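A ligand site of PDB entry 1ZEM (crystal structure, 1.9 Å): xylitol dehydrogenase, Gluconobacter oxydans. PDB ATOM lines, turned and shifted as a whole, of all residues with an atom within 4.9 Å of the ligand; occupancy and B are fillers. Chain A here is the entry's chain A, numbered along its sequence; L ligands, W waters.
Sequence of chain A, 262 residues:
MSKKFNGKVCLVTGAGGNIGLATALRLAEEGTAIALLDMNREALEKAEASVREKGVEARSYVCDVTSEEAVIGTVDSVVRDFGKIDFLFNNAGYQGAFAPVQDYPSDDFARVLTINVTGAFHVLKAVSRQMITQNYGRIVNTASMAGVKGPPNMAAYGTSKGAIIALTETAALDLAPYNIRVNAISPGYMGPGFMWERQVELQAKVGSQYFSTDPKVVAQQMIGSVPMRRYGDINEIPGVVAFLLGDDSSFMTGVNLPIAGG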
ATOM      1  N   GLY A  14      22.720  -8.483 -22.776  1.00  0.00           N
ATOM      2  CA  GLY A  14      23.552  -7.434 -23.360  1.00  0.00           C
ATOM      3  C   GLY A  14      24.863  -7.443 -22.564  1.00  0.00           C
ATOM      4  O   GLY A  14      25.575  -6.431 -22.498  1.00  0.00           O
ATOM      5  N   GLY A  16      27.662  -8.446 -23.038  1.00  0.00           N
ATOM      6  CA  GLY A  16      28.917  -8.229 -23.720  1.00  0.00           C
ATOM      7  C   GLY A  16      29.166  -6.770 -23.917  1.00  0.00           C
ATOM      8  O   GLY A  16      30.292  -6.365 -24.255  1.00  0.00           O
ATOM      9  N   GLY A  17      28.111  -5.970 -23.722  1.00  0.00           N
ATOM     10  CA  GLY A  17      28.201  -4.530 -23.877  1.00  0.00           C
ATOM     11  C   GLY A  17      28.777  -3.797 -22.667  1.00  0.00           C
ATOM     12  O   GLY A  17      29.110  -4.415 -21.669  1.00  0.00           O
ATOM     13  N   ASN A  18      28.875  -2.471 -22.775  1.00  0.00           N
ATOM     14  CA  ASN A  18      29.452  -1.624 -21.709  1.00  0.00           C
ATOM     15  C   ASN A  18      28.774  -1.715 -20.346  1.00  0.00           C
ATOM     16  O   ASN A  18      29.380  -2.075 -19.339  1.00  0.00           O
ATOM     17  CB  ASN A  18      29.425  -0.166 -22.172  1.00  0.00           C
ATOM     18  CG  ASN A  18      30.262   0.069 -23.403  1.00  0.00           C
ATOM     19  OD1 ASN A  18      31.396  -0.393 -23.478  1.00  0.00           O
ATOM     20  ND2 ASN A  18      29.717   0.807 -24.378  1.00  0.00           N
ATOM     21  N   ILE A  19      27.488  -1.381 -20.329  1.00  0.00           N
ATOM     22  CA  ILE A  19      26.751  -1.405 -19.083  1.00  0.00           C
ATOM     23  C   ILE A  19      26.544  -2.790 -18.555  1.00  0.00           C
ATOM     24  O   ILE A  19      26.612  -3.016 -17.344  1.00  0.00           O
ATOM     25  CB  ILE A  19      25.373  -0.681 -19.253  1.00  0.00           C
ATOM     26  CG1 ILE A  19      25.624   0.759 -19.779  1.00  0.00           C
ATOM     27  CG2 ILE A  19      24.581  -0.646 -17.930  1.00  0.00           C
ATOM     28  CD1 ILE A  19      24.379   1.518 -20.230  1.00  0.00           C
ATOM     29  N   GLY A  20      26.321  -3.746 -19.457  1.00  0.00           N
ATOM     30  CA  GLY A  20      26.104  -5.094 -18.965  1.00  0.00           C
ATOM     31  C   GLY A  20      27.377  -5.669 -18.353  1.00  0.00           C
ATOM     32  O   GLY A  20      27.349  -6.321 -17.308  1.00  0.00           O
ATOM     33  N   LEU A  37      24.291 -13.170 -21.172  1.00  0.00           N
ATOM     34  CA  LEU A  37      23.541 -13.373 -22.434  1.00  0.00           C
ATOM     35  C   LEU A  37      23.767 -12.235 -23.457  1.00  0.00           C
ATOM     36  O   LEU A  37      23.667 -11.029 -23.133  1.00  0.00           O
ATOM     37  CB  LEU A  37      22.054 -13.560 -22.090  1.00  0.00           C
ATOM     38  CG  LEU A  37      21.093 -13.936 -23.202  1.00  0.00           C
ATOM     39  CD1 LEU A  37      19.779 -14.335 -22.550  1.00  0.00           C
ATOM     40  CD2 LEU A  37      20.891 -12.757 -24.167  1.00  0.00           C
ATOM     41  N   ASP A  38      24.075 -12.590 -24.702  1.00  0.00           N
ATOM     42  CA  ASP A  38      24.284 -11.570 -25.742  1.00  0.00           C
ATOM     43  C   ASP A  38      24.205 -12.256 -27.084  1.00  0.00           C
ATOM     44  O   ASP A  38      24.235 -13.496 -27.160  1.00  0.00           O
ATOM     45  CB  ASP A  38      25.672 -10.917 -25.619  1.00  0.00           C
ATOM     46  CG  ASP A  38      25.721  -9.500 -26.172  1.00  0.00           C
ATOM     47  OD1 ASP A  38      25.794  -8.549 -25.326  1.00  0.00           O
ATOM     48  OD2 ASP A  38      25.738  -9.296 -27.412  1.00  0.00           O
ATOM     49  N   MET A  39      24.093 -11.463 -28.147  1.00  0.00           N
ATOM     50  CA  MET A  39      24.027 -12.019 -29.482  1.00  0.00           C
ATOM     51  C   MET A  39      25.452 -12.120 -30.077  1.00  0.00           C
ATOM     52  O   MET A  39      25.694 -12.846 -31.045  1.00  0.00           O
ATOM     53  CB  MET A  39      23.143 -11.149 -30.370  1.00  0.00           C
ATOM     54  CG  MET A  39      23.656  -9.737 -30.663  1.00  0.00           C
ATOM     55  SD  MET A  39      22.653  -8.908 -31.937  1.00  0.00           S
ATOM     56  CE  MET A  39      21.791 -10.432 -32.732  1.00  0.00           C
ATOM     57  N   ASN A  40      26.390 -11.385 -29.503  1.00  0.00           N
ATOM     58  CA  ASN A  40      27.752 -11.384 -30.024  1.00  0.00           C
ATOM     59  C   ASN A  40      28.639 -12.293 -29.178  1.00  0.00           C
ATOM     60  O   ASN A  40      28.958 -11.992 -28.037  1.00  0.00           O
ATOM     61  CB  ASN A  40      28.277  -9.950 -30.008  1.00  0.00           C
ATOM     62  CG  ASN A  40      29.744  -9.853 -30.338  1.00  0.00           C
ATOM     63  OD1 ASN A  40      30.574 -10.615 -29.817  1.00  0.00           O
ATOM     64  ND2 ASN A  40      30.087  -8.904 -31.175  1.00  0.00           N
ATOM     65  N   CYS A  63      22.614 -15.727 -27.738  1.00  0.00           N
ATOM     66  CA  CYS A  63      21.166 -15.721 -27.868  1.00  0.00           C
ATOM     67  C   CYS A  63      20.656 -14.383 -28.401  1.00  0.00           C
ATOM     68  O   CYS A  63      21.071 -13.338 -27.910  1.00  0.00           O
ATOM     69  CB  CYS A  63      20.589 -16.016 -26.491  1.00  0.00           C
ATOM     70  SG  CYS A  63      18.743 -15.842 -26.360  1.00  0.00           S
ATOM     71  N   ASP A  64      19.772 -14.400 -29.394  1.00  0.00           N
ATOM     72  CA  ASP A  64      19.196 -13.196 -29.972  1.00  0.00           C
ATOM     73  C   ASP A  64      17.827 -13.001 -29.285  1.00  0.00           C
ATOM     74  O   ASP A  64      16.873 -13.744 -29.565  1.00  0.00           O
ATOM     75  CB  ASP A  64      19.039 -13.401 -31.477  1.00  0.00           C
ATOM     76  CG  ASP A  64      18.232 -12.321 -32.164  1.00  0.00           C
ATOM     77  OD1 ASP A  64      18.130 -12.458 -33.390  1.00  0.00           O
ATOM     78  OD2 ASP A  64      17.689 -11.355 -31.535  1.00  0.00           O
ATOM     79  N   VAL A  65      17.741 -12.052 -28.356  1.00  0.00           N
ATOM     80  CA  VAL A  65      16.498 -11.856 -27.609  1.00  0.00           C
ATOM     81  C   VAL A  65      15.281 -11.639 -28.512  1.00  0.00           C
ATOM     82  O   VAL A  65      14.169 -11.825 -28.058  1.00  0.00           O
ATOM     83  CB  VAL A  65      16.600 -10.704 -26.561  1.00  0.00           C
ATOM     84  CG1 VAL A  65      17.725 -10.968 -25.614  1.00  0.00           C
ATOM     85  CG2 VAL A  65      16.764  -9.395 -27.225  1.00  0.00           C
ATOM     86  N   THR A  66      15.470 -11.308 -29.795  1.00  0.00           N
ATOM     87  CA  THR A  66      14.284 -11.142 -30.648  1.00  0.00           C
ATOM     88  C   THR A  66      13.667 -12.476 -31.055  1.00  0.00           C
ATOM     89  O   THR A  66      12.574 -12.501 -31.606  1.00  0.00           O
ATOM     90  CB  THR A  66      14.543 -10.376 -31.970  1.00  0.00           C
ATOM     91  OG1 THR A  66      15.441 -11.121 -32.800  1.00  0.00           O
ATOM     92  CG2 THR A  66      15.102  -8.969 -31.694  1.00  0.00           C
ATOM     93  N   ASN A  91      18.858  -5.769 -20.093  1.00  0.00           N
ATOM     94  CA  ASN A  91      19.625  -4.655 -20.609  1.00  0.00           C
ATOM     95  C   ASN A  91      20.053  -4.591 -22.077  1.00  0.00           C
ATOM     96  O   ASN A  91      20.368  -3.497 -22.557  1.00  0.00           O
ATOM     97  CB  ASN A  91      20.809  -4.561 -19.592  1.00  0.00           C
ATOM     98  CG  ASN A  91      21.984  -3.796 -20.093  1.00  0.00           C
ATOM     99  OD1 ASN A  91      22.997  -4.398 -20.504  1.00  0.00           O
ATOM    100  ND2 ASN A  91      21.894  -2.469 -20.045  1.00  0.00           N
ATOM    101  N   ALA A  92      20.038  -5.710 -22.800  1.00  0.00           N
ATOM    102  CA  ALA A  92      20.381  -5.654 -24.210  1.00  0.00           C
ATOM    103  C   ALA A  92      19.509  -4.605 -24.904  1.00  0.00           C
ATOM    104  O   ALA A  92      18.330  -4.508 -24.620  1.00  0.00           O
ATOM    105  CB  ALA A  92      20.148  -7.008 -24.871  1.00  0.00           C
ATOM    106  N   GLY A  93      20.108  -3.858 -25.819  1.00  0.00           N
ATOM    107  CA  GLY A  93      19.387  -2.866 -26.572  1.00  0.00           C
ATOM    108  C   GLY A  93      20.188  -2.380 -27.768  1.00  0.00           C
ATOM    109  O   GLY A  93      21.412  -2.601 -27.827  1.00  0.00           O
ATOM    110  N   TYR A  94      19.514  -1.738 -28.705  1.00  0.00           N
ATOM    111  CA  TYR A  94      20.109  -1.182 -29.907  1.00  0.00           C
ATOM    112  C   TYR A  94      19.793   0.308 -29.915  1.00  0.00           C
ATOM    113  O   TYR A  94      18.643   0.717 -29.686  1.00  0.00           O
ATOM    114  CB  TYR A  94      19.520  -1.906 -31.146  1.00  0.00           C
ATOM    115  CG  TYR A  94      19.664  -1.217 -32.475  1.00  0.00           C
ATOM    116  CD1 TYR A  94      20.911  -0.801 -32.946  1.00  0.00           C
ATOM    117  CD2 TYR A  94      18.531  -0.920 -33.240  1.00  0.00           C
ATOM    118  CE1 TYR A  94      21.010  -0.091 -34.163  1.00  0.00           C
ATOM    119  CE2 TYR A  94      18.609  -0.234 -34.409  1.00  0.00           C
ATOM    120  CZ  TYR A  94      19.850   0.189 -34.878  1.00  0.00           C
ATOM    121  OH  TYR A  94      19.899   0.936 -36.018  1.00  0.00           O
ATOM    122  N   ILE A 115      13.826  -5.150 -30.903  1.00  0.00           N
ATOM    123  CA  ILE A 115      14.946  -5.518 -30.005  1.00  0.00           C
ATOM    124  C   ILE A 115      14.766  -4.950 -28.588  1.00  0.00           C
ATOM    125  O   ILE A 115      14.815  -5.700 -27.590  1.00  0.00           O
ATOM    126  CB  ILE A 115      16.270  -4.981 -30.582  1.00  0.00           C
ATOM    127  CG1 ILE A 115      16.603  -5.737 -31.889  1.00  0.00           C
ATOM    128  CG2 ILE A 115      17.405  -5.179 -29.560  1.00  0.00           C
ATOM    129  CD1 ILE A 115      17.659  -5.015 -32.778  1.00  0.00           C
ATOM    130  N   THR A 142      16.579  -1.848 -18.371  1.00  0.00           N
ATOM    131  CA  THR A 142      17.287  -0.618 -18.680  1.00  0.00           C
ATOM    132  C   THR A 142      16.448   0.250 -19.590  1.00  0.00           C
ATOM    133  O   THR A 142      16.236  -0.102 -20.722  1.00  0.00           O
ATOM    134  CB  THR A 142      18.638  -0.922 -19.374  1.00  0.00           C
ATOM    135  OG1 THR A 142      19.388  -1.789 -18.532  1.00  0.00           O
ATOM    136  CG2 THR A 142      19.449   0.367 -19.565  1.00  0.00           C
ATOM    137  N   ALA A 143      15.947   1.390 -19.079  1.00  0.00           N
ATOM    138  CA  ALA A 143      15.199   2.341 -19.902  1.00  0.00           C
ATOM    139  C   ALA A 143      16.247   3.370 -20.380  1.00  0.00           C
ATOM    140  O   ALA A 143      17.330   3.021 -20.835  1.00  0.00           O
ATOM    141  CB  ALA A 143      14.110   3.041 -19.068  1.00  0.00           C
ATOM    142  N   SER A 144      15.965   4.664 -20.203  1.00  0.00           N
ATOM    143  CA  SER A 144      16.892   5.713 -20.644  1.00  0.00           C
ATOM    144  C   SER A 144      16.206   7.042 -20.488  1.00  0.00           C
ATOM    145  O   SER A 144      14.977   7.118 -20.528  1.00  0.00           O
ATOM    146  CB  SER A 144      17.248   5.535 -22.126  1.00  0.00           C
ATOM    147  OG  SER A 144      17.769   6.699 -22.691  1.00  0.00           O
ATOM    148  N   TYR A 157      14.154   5.067 -30.843  1.00  0.00           N
ATOM    149  CA  TYR A 157      14.704   4.750 -29.563  1.00  0.00           C
ATOM    150  C   TYR A 157      13.879   5.327 -28.368  1.00  0.00           C
ATOM    151  O   TYR A 157      13.632   4.631 -27.360  1.00  0.00           O
ATOM    152  CB  TYR A 157      16.158   5.232 -29.526  1.00  0.00           C
ATOM    153  CG  TYR A 157      16.946   4.833 -28.312  1.00  0.00           C
ATOM    154  CD1 TYR A 157      17.538   3.562 -28.210  1.00  0.00           C
ATOM    155  CD2 TYR A 157      17.079   5.719 -27.236  1.00  0.00           C
ATOM    156  CE1 TYR A 157      18.248   3.181 -27.049  1.00  0.00           C
ATOM    157  CE2 TYR A 157      17.785   5.361 -26.076  1.00  0.00           C
ATOM    158  CZ  TYR A 157      18.360   4.090 -25.977  1.00  0.00           C
ATOM    159  OH  TYR A 157      18.989   3.764 -24.806  1.00  0.00           O
ATOM    160  N   LYS A 161      12.052   3.174 -25.358  1.00  0.00           N
ATOM    161  CA  LYS A 161      12.352   3.287 -23.948  1.00  0.00           C
ATOM    162  C   LYS A 161      11.138   3.797 -23.142  1.00  0.00           C
ATOM    163  O   LYS A 161      10.993   3.518 -21.970  1.00  0.00           O
ATOM    164  CB  LYS A 161      13.597   4.158 -23.750  1.00  0.00           C
ATOM    165  CG  LYS A 161      14.879   3.496 -24.419  1.00  0.00           C
ATOM    166  CD  LYS A 161      15.153   2.068 -23.873  1.00  0.00           C
ATOM    167  CE  LYS A 161      16.569   1.606 -24.222  1.00  0.00           C
ATOM    168  NZ  LYS A 161      16.942   0.296 -23.555  1.00  0.00           N
ATOM    169  N   PRO A 187      19.551   5.851 -17.658  1.00  0.00           N
ATOM    170  CA  PRO A 187      20.794   6.605 -17.805  1.00  0.00           C
ATOM    171  C   PRO A 187      20.614   7.778 -18.723  1.00  0.00           C
ATOM    172  O   PRO A 187      19.836   7.732 -19.699  1.00  0.00           O
ATOM    173  CB  PRO A 187      21.783   5.551 -18.370  1.00  0.00           C
ATOM    174  CG  PRO A 187      21.202   4.235 -17.931  1.00  0.00           C
ATOM    175  CD  PRO A 187      19.715   4.438 -18.073  1.00  0.00           C
ATOM    176  N   GLY A 188      21.312   8.863 -18.388  1.00  0.00           N
ATOM    177  CA  GLY A 188      21.320  10.016 -19.241  1.00  0.00           C
ATOM    178  C   GLY A 188      22.529   9.921 -20.180  1.00  0.00           C
ATOM    179  O   GLY A 188      22.637   8.931 -20.886  1.00  0.00           O
ATOM    180  N   TYR A 189      23.379  10.959 -20.202  1.00  0.00           N
ATOM    181  CA  TYR A 189      24.573  10.974 -21.071  1.00  0.00           C
ATOM    182  C   TYR A 189      25.681  10.248 -20.325  1.00  0.00           C
ATOM    183  O   TYR A 189      26.084  10.693 -19.251  1.00  0.00           O
ATOM    184  CB  TYR A 189      25.046  12.397 -21.368  1.00  0.00           C
ATOM    185  CG  TYR A 189      24.152  13.218 -22.288  1.00  0.00           C
ATOM    186  CD1 TYR A 189      23.633  14.453 -21.885  1.00  0.00           C
ATOM    187  CD2 TYR A 189      23.851  12.761 -23.573  1.00  0.00           C
ATOM    188  CE1 TYR A 189      22.816  15.218 -22.756  1.00  0.00           C
ATOM    189  CE2 TYR A 189      23.058  13.508 -24.454  1.00  0.00           C
ATOM    190  CZ  TYR A 189      22.535  14.725 -24.034  1.00  0.00           C
ATOM    191  OH  TYR A 189      21.698  15.377 -24.899  1.00  0.00           O
ATOM    192  N   MET A 190      26.156   9.136 -20.885  1.00  0.00           N
ATOM    193  CA  MET A 190      27.222   8.327 -20.240  1.00  0.00           C
ATOM    194  C   MET A 190      28.401   8.275 -21.193  1.00  0.00           C
ATOM    195  O   MET A 190      28.224   7.941 -22.358  1.00  0.00           O
ATOM    196  CB  MET A 190      26.704   6.906 -19.988  1.00  0.00           C
ATOM    197  CG  MET A 190      25.270   6.882 -19.471  1.00  0.00           C
ATOM    198  SD  MET A 190      25.123   7.756 -17.869  1.00  0.00           S
ATOM    199  CE  MET A 190      26.195   6.627 -16.948  1.00  0.00           C
ATOM    200  N   MET A 195      30.274   4.488 -27.962  1.00  0.00           N
ATOM    201  CA  MET A 195      28.816   4.517 -28.057  1.00  0.00           C
ATOM    202  C   MET A 195      28.399   5.979 -27.768  1.00  0.00           C
ATOM    203  O   MET A 195      27.388   6.476 -28.254  1.00  0.00           O
ATOM    204  CB  MET A 195      28.193   3.585 -27.031  1.00  0.00           C
ATOM    205  CG  MET A 195      27.006   2.795 -27.569  1.00  0.00           C
ATOM    206  SD  MET A 195      27.438   1.850 -29.068  1.00  0.00           S
ATOM    207  CE  MET A 195      26.039   2.312 -30.166  1.00  0.00           C
ATOM    208  N   ILE A 234      30.210   4.986 -16.998  1.00  0.00           N
ATOM    209  CA  ILE A 234      29.484   3.726 -17.039  1.00  0.00           C
ATOM    210  C   ILE A 234      29.558   3.045 -15.678  1.00  0.00           C
ATOM    211  O   ILE A 234      28.626   2.333 -15.289  1.00  0.00           O
ATOM    212  CB  ILE A 234      30.063   2.789 -18.127  1.00  0.00           C
ATOM    213  CG1 ILE A 234      29.632   3.288 -19.488  1.00  0.00           C
ATOM    214  CG2 ILE A 234      29.630   1.387 -17.922  1.00  0.00           C
ATOM    215  CD1 ILE A 234      28.178   3.340 -19.680  1.00  0.00           C
HETATM  216  P1  LIG L   1      26.356  -1.676 -25.781  1.00  0.00           P
HETATM  217  O1  LIG L   1      26.306  -1.655 -27.196  1.00  0.00           O
HETATM  218  O2  LIG L   1      27.796  -1.708 -25.300  1.00  0.00           O
HETATM  219  O3  LIG L   1      25.617  -2.988 -25.225  1.00  0.00           O
HETATM  220  C1  LIG L   1      24.318  -3.399 -25.708  1.00  0.00           C
HETATM  221  C2  LIG L   1      24.603  -4.939 -25.744  1.00  0.00           C
HETATM  222  O4  LIG L   1      23.349  -5.659 -26.121  1.00  0.00           O
HETATM  223  C3  LIG L   1      25.641  -5.415 -26.840  1.00  0.00           C
HETATM  224  O5  LIG L   1      26.502  -6.370 -26.224  1.00  0.00           O
HETATM  225  C4  LIG L   1      24.748  -5.975 -27.968  1.00  0.00           C
HETATM  226  O6  LIG L   1      25.350  -6.970 -28.807  1.00  0.00           O
HETATM  227  C5  LIG L   1      23.543  -6.555 -27.196  1.00  0.00           C
HETATM  228  N1  LIG L   1      22.393  -6.712 -28.084  1.00  0.00           N
HETATM  229  C6  LIG L   1      21.842  -5.903 -29.068  1.00  0.00           C
HETATM  230  N2  LIG L   1      20.841  -6.485 -29.771  1.00  0.00           N
HETATM  231  C7  LIG L   1      20.732  -7.752 -29.188  1.00  0.00           C
HETATM  232  C8  LIG L   1      19.854  -8.843 -29.497  1.00  0.00           C
HETATM  233  N3  LIG L   1      18.923  -8.878 -30.429  1.00  0.00           N
HETATM  234  N4  LIG L   1      19.987 -10.006 -28.727  1.00  0.00           N
HETATM  235  C9  LIG L   1      20.942 -10.083 -27.698  1.00  0.00           C
HETATM  236  N5  LIG L   1      21.812  -9.042 -27.354  1.00  0.00           N
HETATM  237  C10 LIG L   1      21.680  -7.888 -28.135  1.00  0.00           C
HETATM  238  O7  LIG L   1      25.654  -0.409 -25.242  1.00  0.00           O
HETATM  239  P2  LIG L   1      25.287   0.029 -23.808  1.00  0.00           P
HETATM  240  O8  LIG L   1      25.692  -1.018 -22.812  1.00  0.00           O
HETATM  241  O9  LIG L   1      25.385   1.317 -23.281  1.00  0.00           O
HETATM  242  O10 LIG L   1      23.710  -0.425 -23.602  1.00  0.00           O
HETATM  243  C11 LIG L   1      23.140  -1.025 -22.395  1.00  0.00           C
HETATM  244  C12 LIG L   1      21.663  -0.657 -22.341  1.00  0.00           C
HETATM  245  O11 LIG L   1      21.552   0.665 -21.779  1.00  0.00           O
HETATM  246  C13 LIG L   1      20.884  -0.554 -23.706  1.00  0.00           C
HETATM  247  O12 LIG L   1      19.509  -0.979 -23.508  1.00  0.00           O
HETATM  248  C14 LIG L   1      21.007   0.905 -24.031  1.00  0.00           C
HETATM  249  O13 LIG L   1      20.098   1.359 -25.008  1.00  0.00           O
HETATM  250  C15 LIG L   1      20.770   1.499 -22.690  1.00  0.00           C
HETATM  251  N6  LIG L   1      21.280   2.864 -22.496  1.00  0.00           N
HETATM  252  C16 LIG L   1      22.611   3.241 -22.731  1.00  0.00           C
HETATM  253  C17 LIG L   1      22.984   4.561 -22.537  1.00  0.00           C
HETATM  254  C18 LIG L   1      24.433   4.964 -22.804  1.00  0.00           C
HETATM  255  O14 LIG L   1      24.693   6.131 -22.663  1.00  0.00           O
HETATM  256  N7  LIG L   1      25.330   4.081 -23.189  1.00  0.00           N
HETATM  257  C19 LIG L   1      22.014   5.593 -22.104  1.00  0.00           C
HETATM  258  C20 LIG L   1      20.665   5.153 -21.861  1.00  0.00           C
HETATM  259  C21 LIG L   1      20.284   3.790 -22.055  1.00  0.00           C
HETATM  260  O   HOH W   1      23.806  -0.718 -27.975  1.00  0.00           O
HETATM  261  O   HOH W   2      17.004  -3.113 -22.519  1.00  0.00           O
HETATM  262  O   HOH W   3      25.474  -3.477 -22.218  1.00  0.00           O
HETATM  263  O   HOH W   4      28.283   5.470 -24.064  1.00  0.00           O
HETATM  264  O   HOH W   5      27.777   2.646 -24.115  1.00  0.00           O
HETATM  265  O   HOH W   6      23.675  -3.645 -30.774  1.00  0.00           O
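OD1 of Asp 38 lies within hydrogen-bond range of O5 of the ligand (2.5 Å).
O13 of the ligand is in hydrogen-bond range of OH of Tyr 157, at 2.7 Å.
An oxygen (O12) of the ligand is in hydrogen-bond range of the backbone carbonyl oxygen of Asn 91 (2.8 Å).
An oxygen (O2) of the ligand sits at hydrogen-bond distance from the backbone NH of Asn 18.
The side-chain amide nitrogen (ND2) of Asn 18 is in hydrogen-bond range of an oxygen (O2) of the ligand.
The side-chain amino group (NZ) of Lys 161 lies within hydrogen-bond range of an oxygen (O12) of the ligand (2.9 Å).
OD2 of Asp 64 sits at hydrogen-bond distance from N3 of the ligand (3.0 Å).
The backbone NH (N) of Gly 17 lies within hydrogen-bond range of an oxygen (O5) of the ligand (3.0 Å).
The backbone NH of Val 65 sits at hydrogen-bond distance from a nitrogen (N4) of the ligand (3.1 Å).
The backbone NH (N) of Ile 19 is in hydrogen-bond range of an oxygen (O8) of the ligand (3.1 Å).
A nitrogen (N5) of the ligand is in hydrogen-bond range of the backbone NH (N) of Met 39 (3.4 Å).
The backbone carbonyl oxygen (O) of Asp 38 sits at hydrogen-bond distance from the backbone NH (N) of Cys 63 (2.8 Å).
The side-chain carboxylate (OD1) of Asp 38 sits at hydrogen-bond distance from the backbone NH (N) of Gly 16.
The side-chain carboxylate (OD2) of Asp 38 is in hydrogen-bond range of the backbone NH (N) of Asn 40 (3.0 Å).
The side-chain amide nitrogen (ND2) of Asn 91 sits at hydrogen-bond distance from the side-chain hydroxyl (OG1) of Thr 142, at 3.0 Å.
The backbone carbonyl oxygen (O) of Thr 142 sits at hydrogen-bond distance from the side-chain amino group (NZ) of Lys 161.
The side-chain hydroxyl (OG1) of Thr 66 is in hydrogen-bond range of the side-chain carboxylate (OD2) of Asp 64 (2.6 Å).
The backbone NH of Gly 14 sits at hydrogen-bond distance from the backbone carbonyl oxygen of Leu 37, at 2.7 Å.
Merely in contact with the ligand: Thr 142, Cys 63, Ala 143, Gly 14, Met 190, Ser 144, Pro 187, Ala 92, Gly 16, Gly 93, Gly 188 and Ile 115.
Hydrophobic or aromatic side chains that line the ligand: Ile 19, Met 39, Val 65, Ala 92, Ile 115, Tyr 157, Pro 187 and Met 190.
Within 4 Å of the ligand: Gly 14, Gly 16, Gly 17, Asn 18, Ile 19, Asp 38, Met 39, Cys 63, Asp 64, Val 65, Asn 91, Ala 92, Gly 93, Ile 115, Thr 142, Ala 143, Ser 144, Tyr 157, Lys 161, Pro 187, Gly 188 and Met 190.
Water W3 lies within hydrogen-bond range of O8 of the ligand (2.5 Å), N of Gly 20 (2.9 Å), O of Gly 14 (3.0 Å), OD1 of Asn 91 (3.1 Å) and N of Ile 19 (3.5 Å).
Water W1 bridges an oxygen (O1) of the ligand (2.8 Å) and the backbone carbonyl oxygen (O) of Gly 93 (3.0 Å).
Water W5 lies within hydrogen-bond range of the side-chain amide nitrogen of Asn 18 (2.7 Å) and an oxygen (O9) of the ligand (2.9 Å).
Water W4 bridges O of Met 190 (3.0 Å) and N7 of the ligand (3.4 Å).
Water W2 lies within hydrogen-bond range of O of Ala 92 (2.8 Å), O of Asn 91 (3.4 Å) and O12 of the ligand (3.4 Å).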
